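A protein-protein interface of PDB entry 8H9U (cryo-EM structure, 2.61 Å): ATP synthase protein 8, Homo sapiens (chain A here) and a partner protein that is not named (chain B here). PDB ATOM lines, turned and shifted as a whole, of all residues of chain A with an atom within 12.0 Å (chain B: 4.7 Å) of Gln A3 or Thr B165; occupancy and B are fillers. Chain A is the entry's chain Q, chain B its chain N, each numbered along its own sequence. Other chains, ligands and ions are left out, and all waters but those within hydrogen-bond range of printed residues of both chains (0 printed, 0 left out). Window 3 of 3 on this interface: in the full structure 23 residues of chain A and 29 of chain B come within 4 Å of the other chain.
The backbone carbonyl oxygen of Thr B96 lies within hydrogen-bond range of the side-chain amide nitrogen of Gln A3, at 3.0 Å.
The side-chain amide nitrogen (NE2) of Gln A3 sits at hydrogen-bond distance from the side-chain hydroxyl (OG1) of Thr B165, at 3.4 Å.
The backbone carbonyl oxygen of Phe B9 is in hydrogen-bond range of the side-chain amide nitrogen of Gln B97, 2.4 Å away.
OG1 of Thr B161 sits at hydrogen-bond distance from O of Thr B96, 3.0 Å away.
The backbone carbonyl oxygen (O) of Thr B96 sits at hydrogen-bond distance from the side-chain hydroxyl (OG1) of Thr B165 (3.3 Å).
The backbone carbonyl oxygen of Thr B161 lies within hydrogen-bond range of the side-chain hydroxyl of Thr B165 (2.7 Å).
O of Gln A3 sits at hydrogen-bond distance from NE1 of Trp A9, at 2.9 Å.
Among the printed residues, pairs that only touch across the chains: Gln A3 with Phe B9 (3.6 Å), Gln A3 with Leu B98 (3.7 Å), Pro A2 with Phe B9 (3.7 Å) and Gln A3 with Gln B97 (3.95 Å).
Of the printed residues of chain B, Pro A2 touches Phe B9.
Gln A3 touches just these residues of chain B: Phe B9 (3.6 Å), Thr B96 (3.0 Å), Gln B97 (3.95 Å), Leu B98 (3.7 Å) and Thr B165 (3.4 Å).
Trp A9 touches none of the printed residues of chain B.
Pro A10 touches none of the printed residues of chain B.
Of the printed residues of chain A, Phe B9 touches Pro A2 and Gln A3.
Printed residues of chain A within 4 Å of Thr B96: Gln A3 (3.0 Å).
Gln B97 touches one residue of chain A.
No residue of chain A comes within 4 Å of Ala B162.
Thr B165 touches just one residue of chain A: Gln A3 (3.4 Å).
His B168 touches none of the printed residues of chain A.
The nearest residue of chain B that does not touch Gln A3 is Thr B161 (4.4 Å).
The nearest printed residue of chain B that does not touch Pro A2 is Gln B97 (4.6 Å).
Of the 14 printed residues of chain B, 5 touch a printed residue of chain A.
Among the printed residues, 6 pairs touch across the chains.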
ATOM      1  N   MET A   1       6.862  -6.532 -21.949  1.00  0.00           N
ATOM      2  CA  MET A   1       6.250  -5.268 -22.334  1.00  0.00           C
ATOM      3  C   MET A   1       5.216  -5.472 -23.427  1.00  0.00           C
ATOM      4  O   MET A   1       5.561  -5.823 -24.555  1.00  0.00           O
ATOM      5  CB  MET A   1       7.310  -4.274 -22.804  1.00  0.00           C
ATOM      6  CG  MET A   1       8.076  -3.616 -21.680  1.00  0.00           C
ATOM      7  SD  MET A   1       6.978  -2.881 -20.460  1.00  0.00           S
ATOM      8  CE  MET A   1       7.058  -1.156 -20.924  1.00  0.00           C
ATOM      9  N   PRO A   2       3.942  -5.252 -23.094  1.00  0.00           N
ATOM     10  CA  PRO A   2       2.893  -5.355 -24.116  1.00  0.00           C
ATOM     11  C   PRO A   2       3.012  -4.313 -25.208  1.00  0.00           C
ATOM     12  O   PRO A   2       2.490  -4.534 -26.307  1.00  0.00           O
ATOM     13  CB  PRO A   2       1.599  -5.182 -23.313  1.00  0.00           C
ATOM     14  CG  PRO A   2       2.012  -4.472 -22.080  1.00  0.00           C
ATOM     15  CD  PRO A   2       3.390  -4.949 -21.765  1.00  0.00           C
ATOM     16  N   GLN A   3       3.677  -3.185 -24.949  1.00  0.00           N
ATOM     17  CA  GLN A   3       3.933  -2.215 -26.005  1.00  0.00           C
ATOM     18  C   GLN A   3       4.697  -2.824 -27.167  1.00  0.00           C
ATOM     19  O   GLN A   3       4.565  -2.352 -28.301  1.00  0.00           O
ATOM     20  CB  GLN A   3       4.719  -1.029 -25.450  1.00  0.00           C
ATOM     21  CG  GLN A   3       3.884  -0.028 -24.697  1.00  0.00           C
ATOM     22  CD  GLN A   3       3.683  -0.414 -23.256  1.00  0.00           C
ATOM     23  OE1 GLN A   3       3.406  -1.568 -22.944  1.00  0.00           O
ATOM     24  NE2 GLN A   3       3.828   0.551 -22.363  1.00  0.00           N
ATOM     25  N   LEU A   4       5.492  -3.857 -26.911  1.00  0.00           N
ATOM     26  CA  LEU A   4       6.289  -4.511 -27.934  1.00  0.00           C
ATOM     27  C   LEU A   4       5.549  -5.650 -28.611  1.00  0.00           C
ATOM     28  O   LEU A   4       6.126  -6.327 -29.466  1.00  0.00           O
ATOM     29  CB  LEU A   4       7.590  -5.019 -27.320  1.00  0.00           C
ATOM     30  CG  LEU A   4       8.243  -3.944 -26.457  1.00  0.00           C
ATOM     31  CD1 LEU A   4       9.483  -4.478 -25.795  1.00  0.00           C
ATOM     32  CD2 LEU A   4       8.572  -2.722 -27.301  1.00  0.00           C
ATOM     33  N   ASN A   5       4.290  -5.880 -28.249  1.00  0.00           N
ATOM     34  CA  ASN A   5       3.474  -6.874 -28.928  1.00  0.00           C
ATOM     35  C   ASN A   5       3.035  -6.334 -30.280  1.00  0.00           C
ATOM     36  O   ASN A   5       2.010  -5.655 -30.382  1.00  0.00           O
ATOM     37  CB  ASN A   5       2.262  -7.243 -28.074  1.00  0.00           C
ATOM     38  CG  ASN A   5       1.522  -8.440 -28.608  1.00  0.00           C
ATOM     39  OD1 ASN A   5       2.028  -9.162 -29.464  1.00  0.00           O
ATOM     40  ND2 ASN A   5       0.318  -8.665 -28.103  1.00  0.00           N
ATOM     41  N   THR A   6       3.797  -6.638 -31.324  1.00  0.00           N
ATOM     42  CA  THR A   6       3.574  -6.062 -32.642  1.00  0.00           C
ATOM     43  C   THR A   6       2.395  -6.683 -33.376  1.00  0.00           C
ATOM     44  O   THR A   6       2.280  -6.497 -34.591  1.00  0.00           O
ATOM     45  CB  THR A   6       4.836  -6.197 -33.497  1.00  0.00           C
ATOM     46  OG1 THR A   6       5.166  -7.582 -33.647  1.00  0.00           O
ATOM     47  CG2 THR A   6       6.000  -5.471 -32.847  1.00  0.00           C
ATOM     48  N   THR A   7       1.528  -7.423 -32.686  1.00  0.00           N
ATOM     49  CA  THR A   7       0.405  -8.050 -33.372  1.00  0.00           C
ATOM     50  C   THR A   7      -0.838  -7.165 -33.356  1.00  0.00           C
ATOM     51  O   THR A   7      -1.640  -7.208 -34.296  1.00  0.00           O
ATOM     52  CB  THR A   7       0.106  -9.421 -32.758  1.00  0.00           C
ATOM     53  OG1 THR A   7      -0.786 -10.144 -33.612  1.00  0.00           O
ATOM     54  CG2 THR A   7      -0.519  -9.288 -31.385  1.00  0.00           C
ATOM     55  N   VAL A   8      -1.015  -6.351 -32.317  1.00  0.00           N
ATOM     56  CA  VAL A   8      -2.207  -5.519 -32.199  1.00  0.00           C
ATOM     57  C   VAL A   8      -1.873  -4.081 -32.551  1.00  0.00           C
ATOM     58  O   VAL A   8      -2.713  -3.187 -32.404  1.00  0.00           O
ATOM     59  CB  VAL A   8      -2.806  -5.596 -30.787  1.00  0.00           C
ATOM     60  CG1 VAL A   8      -3.194  -7.017 -30.455  1.00  0.00           C
ATOM     61  CG2 VAL A   8      -1.813  -5.062 -29.781  1.00  0.00           C
ATOM     62  N   TRP A   9      -0.643  -3.840 -32.993  1.00  0.00           N
ATOM     63  CA  TRP A   9      -0.285  -2.501 -33.449  1.00  0.00           C
ATOM     64  C   TRP A   9      -1.264  -1.967 -34.487  1.00  0.00           C
ATOM     65  O   TRP A   9      -1.706  -0.815 -34.342  1.00  0.00           O
ATOM     66  CB  TRP A   9       1.158  -2.496 -33.963  1.00  0.00           C
ATOM     67  CG  TRP A   9       2.171  -2.354 -32.869  1.00  0.00           C
ATOM     68  CD1 TRP A   9       2.008  -2.682 -31.559  1.00  0.00           C
ATOM     69  CD2 TRP A   9       3.502  -1.842 -32.991  1.00  0.00           C
ATOM     70  NE1 TRP A   9       3.152  -2.408 -30.855  1.00  0.00           N
ATOM     71  CE2 TRP A   9       4.085  -1.892 -31.713  1.00  0.00           C
ATOM     72  CE3 TRP A   9       4.256  -1.348 -34.057  1.00  0.00           C
ATOM     73  CZ2 TRP A   9       5.385  -1.468 -31.471  1.00  0.00           C
ATOM     74  CZ3 TRP A   9       5.547  -0.928 -33.814  1.00  0.00           C
ATOM     75  CH2 TRP A   9       6.098  -0.991 -32.532  1.00  0.00           C
ATOM     76  N   PRO A  10      -1.677  -2.727 -35.511  1.00  0.00           N
ATOM     77  CA  PRO A  10      -2.661  -2.176 -36.461  1.00  0.00           C
ATOM     78  C   PRO A  10      -3.988  -1.799 -35.827  1.00  0.00           C
ATOM     79  O   PRO A  10      -4.768  -1.056 -36.434  1.00  0.00           O
ATOM     80  CB  PRO A  10      -2.826  -3.307 -37.483  1.00  0.00           C
ATOM     81  CG  PRO A  10      -1.559  -4.063 -37.407  1.00  0.00           C
ATOM     82  CD  PRO A  10      -1.180  -4.039 -35.963  1.00  0.00           C
ATOM     83  N   THR A  11      -4.278  -2.291 -34.625  1.00  0.00           N
ATOM     84  CA  THR A  11      -5.507  -1.894 -33.949  1.00  0.00           C
ATOM     85  C   THR A  11      -5.376  -0.523 -33.293  1.00  0.00           C
ATOM     86  O   THR A  11      -6.391   0.127 -33.028  1.00  0.00           O
ATOM     87  CB  THR A  11      -5.892  -2.966 -32.927  1.00  0.00           C
ATOM     88  OG1 THR A  11      -6.152  -4.195 -33.613  1.00  0.00           O
ATOM     89  CG2 THR A  11      -7.136  -2.579 -32.151  1.00  0.00           C
ATOM     90  N   MET A  12      -4.154  -0.056 -33.048  1.00  0.00           N
ATOM     91  CA  MET A  12      -3.952   1.294 -32.539  1.00  0.00           C
ATOM     92  C   MET A  12      -3.657   2.297 -33.640  1.00  0.00           C
ATOM     93  O   MET A  12      -4.103   3.445 -33.554  1.00  0.00           O
ATOM     94  CB  MET A  12      -2.799   1.326 -31.537  1.00  0.00           C
ATOM     95  CG  MET A  12      -2.888   0.292 -30.452  1.00  0.00           C
ATOM     96  SD  MET A  12      -4.350   0.504 -29.439  1.00  0.00           S
ATOM     97  CE  MET A  12      -4.265  -1.001 -28.490  1.00  0.00           C
ATOM     98  N   ILE A  13      -2.904   1.897 -34.661  1.00  0.00           N
ATOM     99  CA  ILE A  13      -2.505   2.843 -35.693  1.00  0.00           C
ATOM    100  C   ILE A  13      -3.717   3.404 -36.420  1.00  0.00           C
ATOM    101  O   ILE A  13      -3.814   4.616 -36.630  1.00  0.00           O
ATOM    102  CB  ILE A  13      -1.517   2.187 -36.674  1.00  0.00           C
ATOM    103  CG1 ILE A  13      -0.430   1.411 -35.929  1.00  0.00           C
ATOM    104  CG2 ILE A  13      -0.902   3.230 -37.582  1.00  0.00           C
ATOM    105  CD1 ILE A  13       0.332   2.223 -34.933  1.00  0.00           C
ATOM    106  N   PHE B   9      -1.735  -2.023 -19.905  1.00  0.00           N
ATOM    107  CA  PHE B   9      -1.185  -1.596 -21.179  1.00  0.00           C
ATOM    108  C   PHE B   9      -1.459  -2.585 -22.299  1.00  0.00           C
ATOM    109  O   PHE B   9      -1.148  -2.288 -23.457  1.00  0.00           O
ATOM    110  CB  PHE B   9       0.322  -1.359 -21.050  1.00  0.00           C
ATOM    111  CG  PHE B   9       0.706  -0.584 -19.829  1.00  0.00           C
ATOM    112  CD1 PHE B   9       1.281  -1.216 -18.749  1.00  0.00           C
ATOM    113  CD2 PHE B   9       0.484   0.774 -19.759  1.00  0.00           C
ATOM    114  CE1 PHE B   9       1.629  -0.507 -17.626  1.00  0.00           C
ATOM    115  CE2 PHE B   9       0.832   1.483 -18.637  1.00  0.00           C
ATOM    116  CZ  PHE B   9       1.403   0.842 -17.572  1.00  0.00           C
ATOM    117  N   THR B  96       0.007   5.403 -23.756  1.00  0.00           N
ATOM    118  CA  THR B  96       0.993   4.495 -23.187  1.00  0.00           C
ATOM    119  C   THR B  96       1.509   3.492 -24.200  1.00  0.00           C
ATOM    120  O   THR B  96       2.486   2.797 -23.911  1.00  0.00           O
ATOM    121  CB  THR B  96       0.410   3.731 -22.005  1.00  0.00           C
ATOM    122  OG1 THR B  96      -0.614   2.848 -22.473  1.00  0.00           O
ATOM    123  CG2 THR B  96      -0.171   4.680 -20.998  1.00  0.00           C
ATOM    124  N   GLN B  97       0.879   3.390 -25.362  1.00  0.00           N
ATOM    125  CA  GLN B  97       1.302   2.448 -26.382  1.00  0.00           C
ATOM    126  C   GLN B  97       2.371   3.085 -27.252  1.00  0.00           C
ATOM    127  O   GLN B  97       2.194   4.199 -27.746  1.00  0.00           O
ATOM    128  CB  GLN B  97       0.111   2.018 -27.233  1.00  0.00           C
ATOM    129  CG  GLN B  97      -1.007   1.423 -26.424  1.00  0.00           C
ATOM    130  CD  GLN B  97      -0.675   0.039 -25.938  1.00  0.00           C
ATOM    131  OE1 GLN B  97      -0.264  -0.819 -26.715  1.00  0.00           O
ATOM    132  NE2 GLN B  97      -0.841  -0.190 -24.645  1.00  0.00           N
ATOM    133  N   LEU B  98       3.486   2.376 -27.431  1.00  0.00           N
ATOM    134  CA  LEU B  98       4.506   2.859 -28.347  1.00  0.00           C
ATOM    135  C   LEU B  98       4.025   2.828 -29.786  1.00  0.00           C
ATOM    136  O   LEU B  98       4.447   3.668 -30.586  1.00  0.00           O
ATOM    137  CB  LEU B  98       5.780   2.031 -28.208  1.00  0.00           C
ATOM    138  CG  LEU B  98       6.896   2.411 -29.178  1.00  0.00           C
ATOM    139  CD1 LEU B  98       7.572   3.691 -28.737  1.00  0.00           C
ATOM    140  CD2 LEU B  98       7.901   1.287 -29.318  1.00  0.00           C
ATOM    141  N   LEU B 160       6.806  10.448 -24.905  1.00  0.00           N
ATOM    142  CA  LEU B 160       5.399  10.408 -24.533  1.00  0.00           C
ATOM    143  C   LEU B 160       5.032   9.072 -23.905  1.00  0.00           C
ATOM    144  O   LEU B 160       4.426   9.026 -22.833  1.00  0.00           O
ATOM    145  CB  LEU B 160       4.524  10.690 -25.751  1.00  0.00           C
ATOM    146  CG  LEU B 160       3.047  10.860 -25.422  1.00  0.00           C
ATOM    147  CD1 LEU B 160       2.874  11.900 -24.346  1.00  0.00           C
ATOM    148  CD2 LEU B 160       2.286  11.251 -26.657  1.00  0.00           C
ATOM    149  N   THR B 161       5.399   7.968 -24.552  1.00  0.00           N
ATOM    150  CA  THR B 161       5.035   6.665 -24.014  1.00  0.00           C
ATOM    151  C   THR B 161       5.739   6.392 -22.695  1.00  0.00           C
ATOM    152  O   THR B 161       5.120   5.876 -21.764  1.00  0.00           O
ATOM    153  CB  THR B 161       5.333   5.544 -25.008  1.00  0.00           C
ATOM    154  OG1 THR B 161       5.079   4.286 -24.380  1.00  0.00           O
ATOM    155  CG2 THR B 161       6.760   5.573 -25.459  1.00  0.00           C
ATOM    156  N   ALA B 162       7.018   6.741 -22.586  1.00  0.00           N
ATOM    157  CA  ALA B 162       7.749   6.416 -21.369  1.00  0.00           C
ATOM    158  C   ALA B 162       7.380   7.327 -20.213  1.00  0.00           C
ATOM    159  O   ALA B 162       7.592   6.955 -19.056  1.00  0.00           O
ATOM    160  CB  ALA B 162       9.252   6.476 -21.621  1.00  0.00           C
ATOM    161  N   ASN B 163       6.831   8.507 -20.490  1.00  0.00           N
ATOM    162  CA  ASN B 163       6.467   9.419 -19.415  1.00  0.00           C
ATOM    163  C   ASN B 163       5.053   9.146 -18.924  1.00  0.00           C
ATOM    164  O   ASN B 163       4.746   9.332 -17.743  1.00  0.00           O
ATOM    165  CB  ASN B 163       6.601  10.864 -19.885  1.00  0.00           C
ATOM    166  CG  ASN B 163       6.860  11.814 -18.752  1.00  0.00           C
ATOM    167  OD1 ASN B 163       6.464  11.565 -17.617  1.00  0.00           O
ATOM    168  ND2 ASN B 163       7.529  12.917 -19.048  1.00  0.00           N
ATOM    169  N   ILE B 164       4.177   8.709 -19.824  1.00  0.00           N
ATOM    170  CA  ILE B 164       2.798   8.421 -19.443  1.00  0.00           C
ATOM    171  C   ILE B 164       2.696   7.021 -18.852  1.00  0.00           C
ATOM    172  O   ILE B 164       1.894   6.765 -17.949  1.00  0.00           O
ATOM    173  CB  ILE B 164       1.863   8.603 -20.649  1.00  0.00           C
ATOM    174  CG1 ILE B 164       2.012  10.011 -21.214  1.00  0.00           C
ATOM    175  CG2 ILE B 164       0.434   8.388 -20.247  1.00  0.00           C
ATOM    176  CD1 ILE B 164       1.695  11.086 -20.220  1.00  0.00           C
ATOM    177  N   THR B 165       3.511   6.092 -19.354  1.00  0.00           N
ATOM    178  CA  THR B 165       3.525   4.741 -18.808  1.00  0.00           C
ATOM    179  C   THR B 165       4.094   4.728 -17.398  1.00  0.00           C
ATOM    180  O   THR B 165       3.494   4.170 -16.473  1.00  0.00           O
ATOM    181  CB  THR B 165       4.341   3.808 -19.704  1.00  0.00           C
ATOM    182  OG1 THR B 165       3.720   3.711 -20.989  1.00  0.00           O
ATOM    183  CG2 THR B 165       4.422   2.437 -19.094  1.00  0.00           C
ATOM    184  N   ALA B 166       5.264   5.343 -17.224  1.00  0.00           N
ATOM    185  CA  ALA B 166       5.896   5.392 -15.913  1.00  0.00           C
ATOM    186  C   ALA B 166       4.996   6.081 -14.899  1.00  0.00           C
ATOM    187  O   ALA B 166       4.917   5.673 -13.737  1.00  0.00           O
ATOM    188  CB  ALA B 166       7.244   6.103 -16.011  1.00  0.00           C
ATOM    189  N   GLY B 167       4.309   7.134 -15.322  1.00  0.00           N
ATOM    190  CA  GLY B 167       3.378   7.815 -14.451  1.00  0.00           C
ATOM    191  C   GLY B 167       2.233   6.932 -14.006  1.00  0.00           C
ATOM    192  O   GLY B 167       1.866   6.934 -12.830  1.00  0.00           O
ATOM    193  N   HIS B 168       1.657   6.170 -14.936  1.00  0.00           N
ATOM    194  CA  HIS B 168       0.544   5.294 -14.587  1.00  0.00           C
ATOM    195  C   HIS B 168       1.005   4.133 -13.721  1.00  0.00           C
ATOM    196  O   HIS B 168       0.340   3.768 -12.746  1.00  0.00           O
ATOM    197  CB  HIS B 168      -0.131   4.781 -15.854  1.00  0.00           C
ATOM    198  CG  HIS B 168      -1.015   5.791 -16.506  1.00  0.00           C
ATOM    199  ND1 HIS B 168      -0.542   6.732 -17.392  1.00  0.00           N
ATOM    200  CD2 HIS B 168      -2.343   6.016 -16.390  1.00  0.00           C
ATOM    201  CE1 HIS B 168      -1.542   7.494 -17.796  1.00  0.00           C
ATOM    202  NE2 HIS B 168      -2.646   7.078 -17.205  1.00  0.00           N
ATOM    203  N   LEU B 169       2.138   3.531 -14.073  1.00  0.00           N
ATOM    204  CA  LEU B 169       2.646   2.414 -13.287  1.00  0.00           C
ATOM    205  C   LEU B 169       2.985   2.858 -11.874  1.00  0.00           C
ATOM    206  O   LEU B 169       2.729   2.134 -10.907  1.00  0.00           O
ATOM    207  CB  LEU B 169       3.868   1.813 -13.971  1.00  0.00           C
ATOM    208  CG  LEU B 169       4.199   0.353 -13.677  1.00  0.00           C
ATOM    209  CD1 LEU B 169       4.996  -0.213 -14.825  1.00  0.00           C
ATOM    210  CD2 LEU B 169       4.947   0.172 -12.370  1.00  0.00           C
